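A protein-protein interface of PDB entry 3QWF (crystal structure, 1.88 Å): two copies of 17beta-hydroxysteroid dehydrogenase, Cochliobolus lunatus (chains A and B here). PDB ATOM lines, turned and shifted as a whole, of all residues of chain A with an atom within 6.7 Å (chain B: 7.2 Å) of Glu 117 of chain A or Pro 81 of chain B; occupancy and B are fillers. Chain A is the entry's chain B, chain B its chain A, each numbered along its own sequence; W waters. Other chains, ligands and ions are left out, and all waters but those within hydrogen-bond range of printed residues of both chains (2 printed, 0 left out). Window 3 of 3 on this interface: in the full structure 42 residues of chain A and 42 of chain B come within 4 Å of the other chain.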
ATOM      1  N   VAL A 115     -24.252 -17.986 -18.338  1.00  0.00           N
ATOM      2  CA  VAL A 115     -25.585 -17.909 -17.746  1.00  0.00           C
ATOM      3  C   VAL A 115     -25.530 -18.305 -16.262  1.00  0.00           C
ATOM      4  O   VAL A 115     -24.993 -19.358 -15.895  1.00  0.00           O
ATOM      5  CB  VAL A 115     -26.644 -18.720 -18.533  1.00  0.00           C
ATOM      6  CG1 VAL A 115     -28.013 -18.637 -17.859  1.00  0.00           C
ATOM      7  CG2 VAL A 115     -26.734 -18.215 -19.980  1.00  0.00           C
ATOM      8  N   THR A 116     -26.053 -17.413 -15.426  1.00  0.00           N
ATOM      9  CA  THR A 116     -26.046 -17.582 -13.983  1.00  0.00           C
ATOM     10  C   THR A 116     -27.342 -18.249 -13.524  1.00  0.00           C
ATOM     11  O   THR A 116     -28.337 -18.259 -14.245  1.00  0.00           O
ATOM     12  CB  THR A 116     -25.949 -16.217 -13.272  1.00  0.00           C
ATOM     13  OG1 THR A 116     -27.081 -15.419 -13.640  1.00  0.00           O
ATOM     14  CG2 THR A 116     -24.654 -15.478 -13.638  1.00  0.00           C
ATOM     15  N   GLU A 117     -27.324 -18.788 -12.306  1.00  0.00           N
ATOM     16  CA  GLU A 117     -28.544 -19.251 -11.649  1.00  0.00           C
ATOM     17  C   GLU A 117     -29.572 -18.131 -11.591  1.00  0.00           C
ATOM     18  O   GLU A 117     -30.753 -18.347 -11.846  1.00  0.00           O
ATOM     19  CB  GLU A 117     -28.235 -19.681 -10.217  1.00  0.00           C
ATOM     20  CG  GLU A 117     -27.560 -21.023 -10.089  1.00  0.00           C
ATOM     21  CD  GLU A 117     -27.576 -21.504  -8.654  1.00  0.00           C
ATOM     22  OE1 GLU A 117     -28.674 -21.655  -8.088  1.00  0.00           O
ATOM     23  OE2 GLU A 117     -26.500 -21.727  -8.090  1.00  0.00           O
ATOM     24  N   GLU A 118     -29.110 -16.935 -11.252  1.00  0.00           N
ATOM     25  CA  GLU A 118     -29.989 -15.784 -11.106  1.00  0.00           C
ATOM     26  C   GLU A 118     -30.720 -15.472 -12.414  1.00  0.00           C
ATOM     27  O   GLU A 118     -31.918 -15.220 -12.400  1.00  0.00           O
ATOM     28  CB  GLU A 118     -29.217 -14.567 -10.585  1.00  0.00           C
ATOM     29  CG  GLU A 118     -28.830 -14.672  -9.112  1.00  0.00           C
ATOM     30  CD  GLU A 118     -27.502 -15.397  -8.856  1.00  0.00           C
ATOM     31  OE1 GLU A 118     -26.998 -16.150  -9.732  1.00  0.00           O
ATOM     32  OE2 GLU A 118     -26.958 -15.202  -7.747  1.00  0.00           O
ATOM     33  N   GLU A 119     -30.008 -15.533 -13.537  1.00  0.00           N
ATOM     34  CA  GLU A 119     -30.616 -15.247 -14.837  1.00  0.00           C
ATOM     35  C   GLU A 119     -31.556 -16.365 -15.297  1.00  0.00           C
ATOM     36  O   GLU A 119     -32.665 -16.085 -15.774  1.00  0.00           O
ATOM     37  CB  GLU A 119     -29.537 -14.919 -15.880  1.00  0.00           C
ATOM     38  CG  GLU A 119     -30.051 -14.460 -17.252  1.00  0.00           C
ATOM     39  CD  GLU A 119     -30.775 -13.106 -17.246  1.00  0.00           C
ATOM     40  OE1 GLU A 119     -30.780 -12.402 -16.219  1.00  0.00           O
ATOM     41  OE2 GLU A 119     -31.345 -12.743 -18.296  1.00  0.00           O
ATOM     42  N   PHE A 120     -31.140 -17.624 -15.128  1.00  0.00           N
ATOM     43  CA  PHE A 120     -32.035 -18.733 -15.430  1.00  0.00           C
ATOM     44  C   PHE A 120     -33.379 -18.504 -14.735  1.00  0.00           C
ATOM     45  O   PHE A 120     -34.433 -18.534 -15.372  1.00  0.00           O
ATOM     46  CB  PHE A 120     -31.463 -20.104 -15.028  1.00  0.00           C
ATOM     47  CG  PHE A 120     -32.339 -21.259 -15.458  1.00  0.00           C
ATOM     48  CD1 PHE A 120     -33.553 -21.516 -14.821  1.00  0.00           C
ATOM     49  CD2 PHE A 120     -31.960 -22.074 -16.526  1.00  0.00           C
ATOM     50  CE1 PHE A 120     -34.383 -22.567 -15.242  1.00  0.00           C
ATOM     51  CE2 PHE A 120     -32.761 -23.125 -16.947  1.00  0.00           C
ATOM     52  CZ  PHE A 120     -33.990 -23.366 -16.309  1.00  0.00           C
ATOM     53  N   ASP A 121     -33.319 -18.241 -13.431  1.00  0.00           N
ATOM     54  CA  ASP A 121     -34.524 -18.079 -12.622  1.00  0.00           C
ATOM     55  C   ASP A 121     -35.350 -16.841 -12.970  1.00  0.00           C
ATOM     56  O   ASP A 121     -36.578 -16.906 -12.982  1.00  0.00           O
ATOM     57  CB  ASP A 121     -34.170 -18.121 -11.132  1.00  0.00           C
ATOM     58  CG  ASP A 121     -33.686 -19.498 -10.693  1.00  0.00           C
ATOM     59  OD1 ASP A 121     -34.045 -20.512 -11.352  1.00  0.00           O
ATOM     60  OD2 ASP A 121     -32.946 -19.563  -9.698  1.00  0.00           O
ATOM     61  N   ARG A 122     -34.680 -15.722 -13.235  1.00  0.00           N
ATOM     62  CA  ARG A 122     -35.361 -14.512 -13.704  1.00  0.00           C
ATOM     63  C   ARG A 122     -36.247 -14.799 -14.920  1.00  0.00           C
ATOM     64  O   ARG A 122     -37.379 -14.320 -14.999  1.00  0.00           O
ATOM     65  CB  ARG A 122     -34.349 -13.395 -14.027  1.00  0.00           C
ATOM     66  CG  ARG A 122     -35.001 -12.036 -14.328  1.00  0.00           C
ATOM     67  CD  ARG A 122     -33.970 -10.963 -14.726  1.00  0.00           C
ATOM     68  NE  ARG A 122     -33.426 -11.180 -16.069  1.00  0.00           N
ATOM     69  CZ  ARG A 122     -33.996 -10.750 -17.194  1.00  0.00           C
ATOM     70  NH1 ARG A 122     -35.147 -10.079 -17.160  1.00  0.00           N
ATOM     71  NH2 ARG A 122     -33.417 -10.994 -18.363  1.00  0.00           N
ATOM     72  N   ALA B  75     -23.508 -36.360  -6.218  1.00  0.00           N
ATOM     73  CA  ALA B  75     -23.884 -34.971  -6.436  1.00  0.00           C
ATOM     74  C   ALA B  75     -25.382 -34.883  -6.747  1.00  0.00           C
ATOM     75  O   ALA B  75     -25.897 -35.578  -7.636  1.00  0.00           O
ATOM     76  CB  ALA B  75     -23.060 -34.349  -7.572  1.00  0.00           C
ATOM     77  N   ASP B  76     -26.065 -34.018  -6.012  1.00  0.00           N
ATOM     78  CA  ASP B  76     -27.457 -33.684  -6.277  1.00  0.00           C
ATOM     79  C   ASP B  76     -27.499 -32.702  -7.449  1.00  0.00           C
ATOM     80  O   ASP B  76     -27.122 -31.536  -7.307  1.00  0.00           O
ATOM     81  CB  ASP B  76     -28.080 -33.069  -5.017  1.00  0.00           C
ATOM     82  CG  ASP B  76     -29.567 -32.765  -5.169  1.00  0.00           C
ATOM     83  OD1 ASP B  76     -30.135 -32.939  -6.276  1.00  0.00           O
ATOM     84  OD2 ASP B  76     -30.171 -32.344  -4.158  1.00  0.00           O
ATOM     85  N   ARG B  78     -29.857 -31.142  -8.760  1.00  0.00           N
ATOM     86  CA  ARG B  78     -30.666 -29.946  -8.507  1.00  0.00           C
ATOM     87  C   ARG B  78     -29.802 -28.783  -8.013  1.00  0.00           C
ATOM     88  O   ARG B  78     -30.156 -27.618  -8.197  1.00  0.00           O
ATOM     89  CB  ARG B  78     -31.774 -30.215  -7.485  1.00  0.00           C
ATOM     90  CG  ARG B  78     -32.916 -31.058  -8.013  1.00  0.00           C
ATOM     91  CD  ARG B  78     -34.091 -31.064  -7.040  1.00  0.00           C
ATOM     92  NE  ARG B  78     -35.215 -31.742  -7.681  1.00  0.00           N
ATOM     93  CZ  ARG B  78     -35.466 -33.044  -7.589  1.00  0.00           C
ATOM     94  NH1 ARG B  78     -34.689 -33.831  -6.851  1.00  0.00           N
ATOM     95  NH2 ARG B  78     -36.500 -33.560  -8.238  1.00  0.00           N
ATOM     96  N   GLN B  79     -28.679 -29.102  -7.376  1.00  0.00           N
ATOM     97  CA  GLN B  79     -27.825 -28.071  -6.792  1.00  0.00           C
ATOM     98  C   GLN B  79     -26.697 -27.710  -7.739  1.00  0.00           C
ATOM     99  O   GLN B  79     -25.787 -28.522  -7.960  1.00  0.00           O
ATOM    100  CB  GLN B  79     -27.255 -28.535  -5.445  1.00  0.00           C
ATOM    101  CG  GLN B  79     -28.225 -29.332  -4.579  1.00  0.00           C
ATOM    102  CD  GLN B  79     -29.491 -28.560  -4.246  1.00  0.00           C
ATOM    103  OE1 GLN B  79     -29.446 -27.355  -4.005  1.00  0.00           O
ATOM    104  NE2 GLN B  79     -30.625 -29.254  -4.230  1.00  0.00           N
ATOM    105  N   VAL B  80     -26.743 -26.493  -8.283  1.00  0.00           N
ATOM    106  CA  VAL B  80     -25.713 -26.016  -9.226  1.00  0.00           C
ATOM    107  C   VAL B  80     -24.277 -26.054  -8.646  1.00  0.00           C
ATOM    108  O   VAL B  80     -23.343 -26.405  -9.371  1.00  0.00           O
ATOM    109  CB  VAL B  80     -26.065 -24.625  -9.838  1.00  0.00           C
ATOM    110  CG1 VAL B  80     -24.919 -24.084 -10.694  1.00  0.00           C
ATOM    111  CG2 VAL B  80     -27.370 -24.733 -10.690  1.00  0.00           C
ATOM    112  N   PRO B  81     -24.100 -25.724  -7.345  1.00  0.00           N
ATOM    113  CA  PRO B  81     -22.752 -25.863  -6.776  1.00  0.00           C
ATOM    114  C   PRO B  81     -22.241 -27.311  -6.718  1.00  0.00           C
ATOM    115  O   PRO B  81     -21.033 -27.523  -6.783  1.00  0.00           O
ATOM    116  CB  PRO B  81     -22.902 -25.272  -5.374  1.00  0.00           C
ATOM    117  CG  PRO B  81     -23.995 -24.266  -5.537  1.00  0.00           C
ATOM    118  CD  PRO B  81     -24.975 -24.951  -6.444  1.00  0.00           C
ATOM    119  N   GLU B  82     -23.147 -28.289  -6.646  1.00  0.00           N
ATOM    120  CA  GLU B  82     -22.743 -29.701  -6.676  1.00  0.00           C
ATOM    121  C   GLU B  82     -22.436 -30.192  -8.090  1.00  0.00           C
ATOM    122  O   GLU B  82     -21.635 -31.120  -8.263  1.00  0.00           O
ATOM    123  CB  GLU B  82     -23.760 -30.606  -5.972  1.00  0.00           C
ATOM    124  CG  GLU B  82     -23.776 -30.429  -4.454  1.00  0.00           C
ATOM    125  CD  GLU B  82     -24.715 -31.384  -3.753  1.00  0.00           C
ATOM    126  OE1 GLU B  82     -24.717 -32.591  -4.078  1.00  0.00           O
ATOM    127  OE2 GLU B  82     -25.457 -30.923  -2.862  1.00  0.00           O
ATOM    128  N   ILE B  83     -23.040 -29.557  -9.096  1.00  0.00           N
ATOM    129  CA  ILE B  83     -22.712 -29.862 -10.494  1.00  0.00           C
ATOM    130  C   ILE B  83     -21.280 -29.404 -10.762  1.00  0.00           C
ATOM    131  O   ILE B  83     -20.474 -30.155 -11.313  1.00  0.00           O
ATOM    132  CB  ILE B  83     -23.677 -29.192 -11.493  1.00  0.00           C
ATOM    133  CG1 ILE B  83     -25.125 -29.625 -11.212  1.00  0.00           C
ATOM    134  CG2 ILE B  83     -23.281 -29.540 -12.939  1.00  0.00           C
ATOM    135  CD1 ILE B  83     -26.181 -28.875 -12.039  1.00  0.00           C
ATOM    136  N   VAL B  84     -20.982 -28.172 -10.351  1.00  0.00           N
ATOM    137  CA  VAL B  84     -19.641 -27.592 -10.444  1.00  0.00           C
ATOM    138  C   VAL B  84     -18.611 -28.529  -9.803  1.00  0.00           C
ATOM    139  O   VAL B  84     -17.627 -28.921 -10.448  1.00  0.00           O
ATOM    140  CB  VAL B  84     -19.592 -26.183  -9.775  1.00  0.00           C
ATOM    141  CG1 VAL B  84     -18.170 -25.616  -9.773  1.00  0.00           C
ATOM    142  CG2 VAL B  84     -20.552 -25.223 -10.474  1.00  0.00           C
ATOM    143  N   LYS B  85     -18.864 -28.894  -8.545  1.00  0.00           N
ATOM    144  CA  LYS B  85     -18.046 -29.859  -7.806  1.00  0.00           C
ATOM    145  C   LYS B  85     -17.837 -31.171  -8.559  1.00  0.00           C
ATOM    146  O   LYS B  85     -16.711 -31.657  -8.657  1.00  0.00           O
ATOM    147  CB  LYS B  85     -18.660 -30.154  -6.429  1.00  0.00           C
ATOM    148  CG  LYS B  85     -18.536 -29.021  -5.408  1.00  0.00           C
ATOM    149  CD  LYS B  85     -17.275 -29.113  -4.570  1.00  0.00           C
ATOM    150  CE  LYS B  85     -16.853 -27.731  -4.063  1.00  0.00           C
ATOM    151  NZ  LYS B  85     -16.830 -26.748  -5.203  1.00  0.00           N
ATOM    152  N   LEU B  86     -18.931 -31.730  -9.077  1.00  0.00           N
ATOM    153  CA  LEU B  86     -18.918 -32.997  -9.803  1.00  0.00           C
ATOM    154  C   LEU B  86     -17.970 -32.940 -11.002  1.00  0.00           C
ATOM    155  O   LEU B  86     -17.099 -33.802 -11.161  1.00  0.00           O
ATOM    156  CB  LEU B  86     -20.346 -33.385 -10.248  1.00  0.00           C
ATOM    157  CG  LEU B  86     -20.499 -34.533 -11.252  1.00  0.00           C
ATOM    158  CD1 LEU B  86     -20.001 -35.861 -10.689  1.00  0.00           C
ATOM    159  CD2 LEU B  86     -21.946 -34.653 -11.739  1.00  0.00           C
ATOM    160  N   ASP B  88     -15.646 -30.555 -11.590  1.00  0.00           N
ATOM    161  CA  ASP B  88     -14.309 -30.273 -11.041  1.00  0.00           C
ATOM    162  C   ASP B  88     -13.581 -31.552 -10.654  1.00  0.00           C
ATOM    163  O   ASP B  88     -12.412 -31.733 -11.007  1.00  0.00           O
ATOM    164  CB  ASP B  88     -14.390 -29.385  -9.793  1.00  0.00           C
ATOM    165  CG  ASP B  88     -14.608 -27.911 -10.117  1.00  0.00           C
ATOM    166  OD1 ASP B  88     -14.687 -27.526 -11.313  1.00  0.00           O
ATOM    167  OD2 ASP B  88     -14.695 -27.134  -9.145  1.00  0.00           O
ATOM    168  N   ARG B 129     -33.756 -27.093 -15.303  1.00  0.00           N
ATOM    169  CA  ARG B 129     -32.713 -26.253 -14.725  1.00  0.00           C
ATOM    170  C   ARG B 129     -31.440 -27.051 -14.493  1.00  0.00           C
ATOM    171  O   ARG B 129     -30.344 -26.601 -14.859  1.00  0.00           O
ATOM    172  CB  ARG B 129     -33.220 -25.663 -13.402  1.00  0.00           C
ATOM    173  CG  ARG B 129     -32.412 -24.492 -12.855  1.00  0.00           C
ATOM    174  CD  ARG B 129     -33.048 -24.079 -11.533  1.00  0.00           C
ATOM    175  NE  ARG B 129     -32.473 -22.885 -10.943  1.00  0.00           N
ATOM    176  CZ  ARG B 129     -31.401 -22.874 -10.156  1.00  0.00           C
ATOM    177  NH1 ARG B 129     -30.758 -24.007  -9.884  1.00  0.00           N
ATOM    178  NH2 ARG B 129     -30.970 -21.717  -9.642  1.00  0.00           N
ATOM    179  N   PHE B 132     -29.756 -27.907 -17.768  1.00  0.00           N
ATOM    180  CA  PHE B 132     -29.180 -26.696 -18.343  1.00  0.00           C
ATOM    181  C   PHE B 132     -27.793 -26.432 -17.742  1.00  0.00           C
ATOM    182  O   PHE B 132     -26.834 -26.130 -18.464  1.00  0.00           O
ATOM    183  CB  PHE B 132     -30.107 -25.494 -18.109  1.00  0.00           C
ATOM    184  CG  PHE B 132     -29.553 -24.198 -18.638  1.00  0.00           C
ATOM    185  CD1 PHE B 132     -28.662 -23.446 -17.875  1.00  0.00           C
ATOM    186  CD2 PHE B 132     -29.930 -23.733 -19.899  1.00  0.00           C
ATOM    187  CE1 PHE B 132     -28.128 -22.257 -18.381  1.00  0.00           C
ATOM    188  CE2 PHE B 132     -29.407 -22.547 -20.412  1.00  0.00           C
ATOM    189  CZ  PHE B 132     -28.508 -21.810 -19.658  1.00  0.00           C
ATOM    190  N   PHE B 133     -27.687 -26.557 -16.420  1.00  0.00           N
ATOM    191  CA  PHE B 133     -26.431 -26.274 -15.748  1.00  0.00           C
ATOM    192  C   PHE B 133     -25.407 -27.386 -15.859  1.00  0.00           C
ATOM    193  O   PHE B 133     -24.205 -27.132 -15.787  1.00  0.00           O
ATOM    194  CB  PHE B 133     -26.668 -25.801 -14.311  1.00  0.00           C
ATOM    195  CG  PHE B 133     -27.213 -24.419 -14.267  1.00  0.00           C
ATOM    196  CD1 PHE B 133     -26.390 -23.337 -14.577  1.00  0.00           C
ATOM    197  CD2 PHE B 133     -28.552 -24.195 -14.020  1.00  0.00           C
ATOM    198  CE1 PHE B 133     -26.896 -22.050 -14.596  1.00  0.00           C
ATOM    199  CE2 PHE B 133     -29.065 -22.904 -14.014  1.00  0.00           C
ATOM    200  CZ  PHE B 133     -28.231 -21.827 -14.318  1.00  0.00           C
ATOM    201  N   ARG B 136     -23.908 -26.272 -19.019  1.00  0.00           N
ATOM    202  CA  ARG B 136     -22.964 -25.158 -18.734  1.00  0.00           C
ATOM    203  C   ARG B 136     -21.624 -25.643 -18.186  1.00  0.00           C
ATOM    204  O   ARG B 136     -20.566 -25.213 -18.660  1.00  0.00           O
ATOM    205  CB  ARG B 136     -23.582 -24.145 -17.765  1.00  0.00           C
ATOM    206  CG  ARG B 136     -22.755 -22.867 -17.571  1.00  0.00           C
ATOM    207  CD  ARG B 136     -23.261 -22.050 -16.388  1.00  0.00           C
ATOM    208  NE  ARG B 136     -22.744 -22.575 -15.128  1.00  0.00           N
ATOM    209  CZ  ARG B 136     -22.912 -22.004 -13.936  1.00  0.00           C
ATOM    210  NH1 ARG B 136     -23.597 -20.870 -13.815  1.00  0.00           N
ATOM    211  NH2 ARG B 136     -22.391 -22.573 -12.858  1.00  0.00           N
HETATM  212  O   HOH W   1     -24.461 -19.321 -11.499  1.00  0.00           O
HETATM  213  O   HOH W   2     -28.813 -24.648  -7.562  1.00  0.00           O
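The side-chain carboxylate (OE1) of Glu 117 of chain A lies within salt-bridge range of the guanidinium group (NH2) of Arg 129 of chain B, at 2.8 Å.
The guanidinium group (NH1) of Arg 136 of chain B sits at hydrogen-bond distance from the backbone carbonyl oxygen (O) of Val 115 of chain A (2.9 Å).
The side-chain carboxylate (OD1) of Asp 121 of chain A lies within salt-bridge range of the guanidinium group (NE) of Arg 129 of chain B (2.9 Å).
The side-chain hydroxyl of Thr 116 of chain A lies close to the backbone NH of Glu 118 of chain A (3.5 Å).
The side-chain hydroxyl (OG1) of Thr 116 of chain A lies within hydrogen-bond range of the backbone NH (N) of Glu 119 of chain A (2.9 Å).
Among the printed residues, merely in contact across the chains: Glu 117 of chain A with Val 80 of chain B, Phe 120 of chain A with Arg 129 of chain B, Val 115 of chain A with Phe 133 of chain B, Thr 116 of chain A with Phe 133 of chain B, Val 115 of chain A with Phe 132 of chain B, Glu 117 of chain A with Phe 133 of chain B, Phe 120 of chain A with Phe 133 of chain B, Phe 120 of chain A with Phe 132 of chain B and Glu 117 of chain A with Pro 81 of chain B.
Glu 117 of chain A touches just these residues of chain B: Val 80, Pro 81, Arg 129 and Phe 133.
Printed residues of chain B within 4 Å of Phe 120 of chain A: Arg 129, Phe 132 and Phe 133.
Printed residues of chain A within 4 Å of Val 80 of chain B: Glu 117.
Of chain A, only Glu 117 comes within 4 Å of Pro 81 of chain B.
The nearest residue of chain B that does not touch Glu 117 of chain A is Arg 136 of chain B (4.5 Å).
The nearest printed residue of chain A that does not touch Pro 81 of chain B is Glu 118 of chain A (9.6 Å).
Of the 8 printed residues of chain A, 5 touch a printed residue of chain B.
Hydrophobic or aromatic side chains of chain A that line the printed part of chain B: Val 115 and Phe 120.
Of the 16 printed residues of chain B, 6 touch a printed residue of chain A.
Hydrophobic or aromatic side chains of chain B within 4 Å of the printed part of chain A: Val 80, Pro 81, Phe 132 and Phe 133.
No position is printed for both chains.
Water W2 lies within hydrogen-bond range of the backbone NH of Val 80 of chain B, the side-chain carboxylate of Glu 117 of chain A, the guanidinium group of Arg 129 of chain B and the backbone carbonyl oxygen of Arg 78 of chain B.
Water W1 lies within hydrogen-bond range of NH1 of Arg 136 of chain B (2.9 Å) and N of Glu 117 of chain A (3.0 Å).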
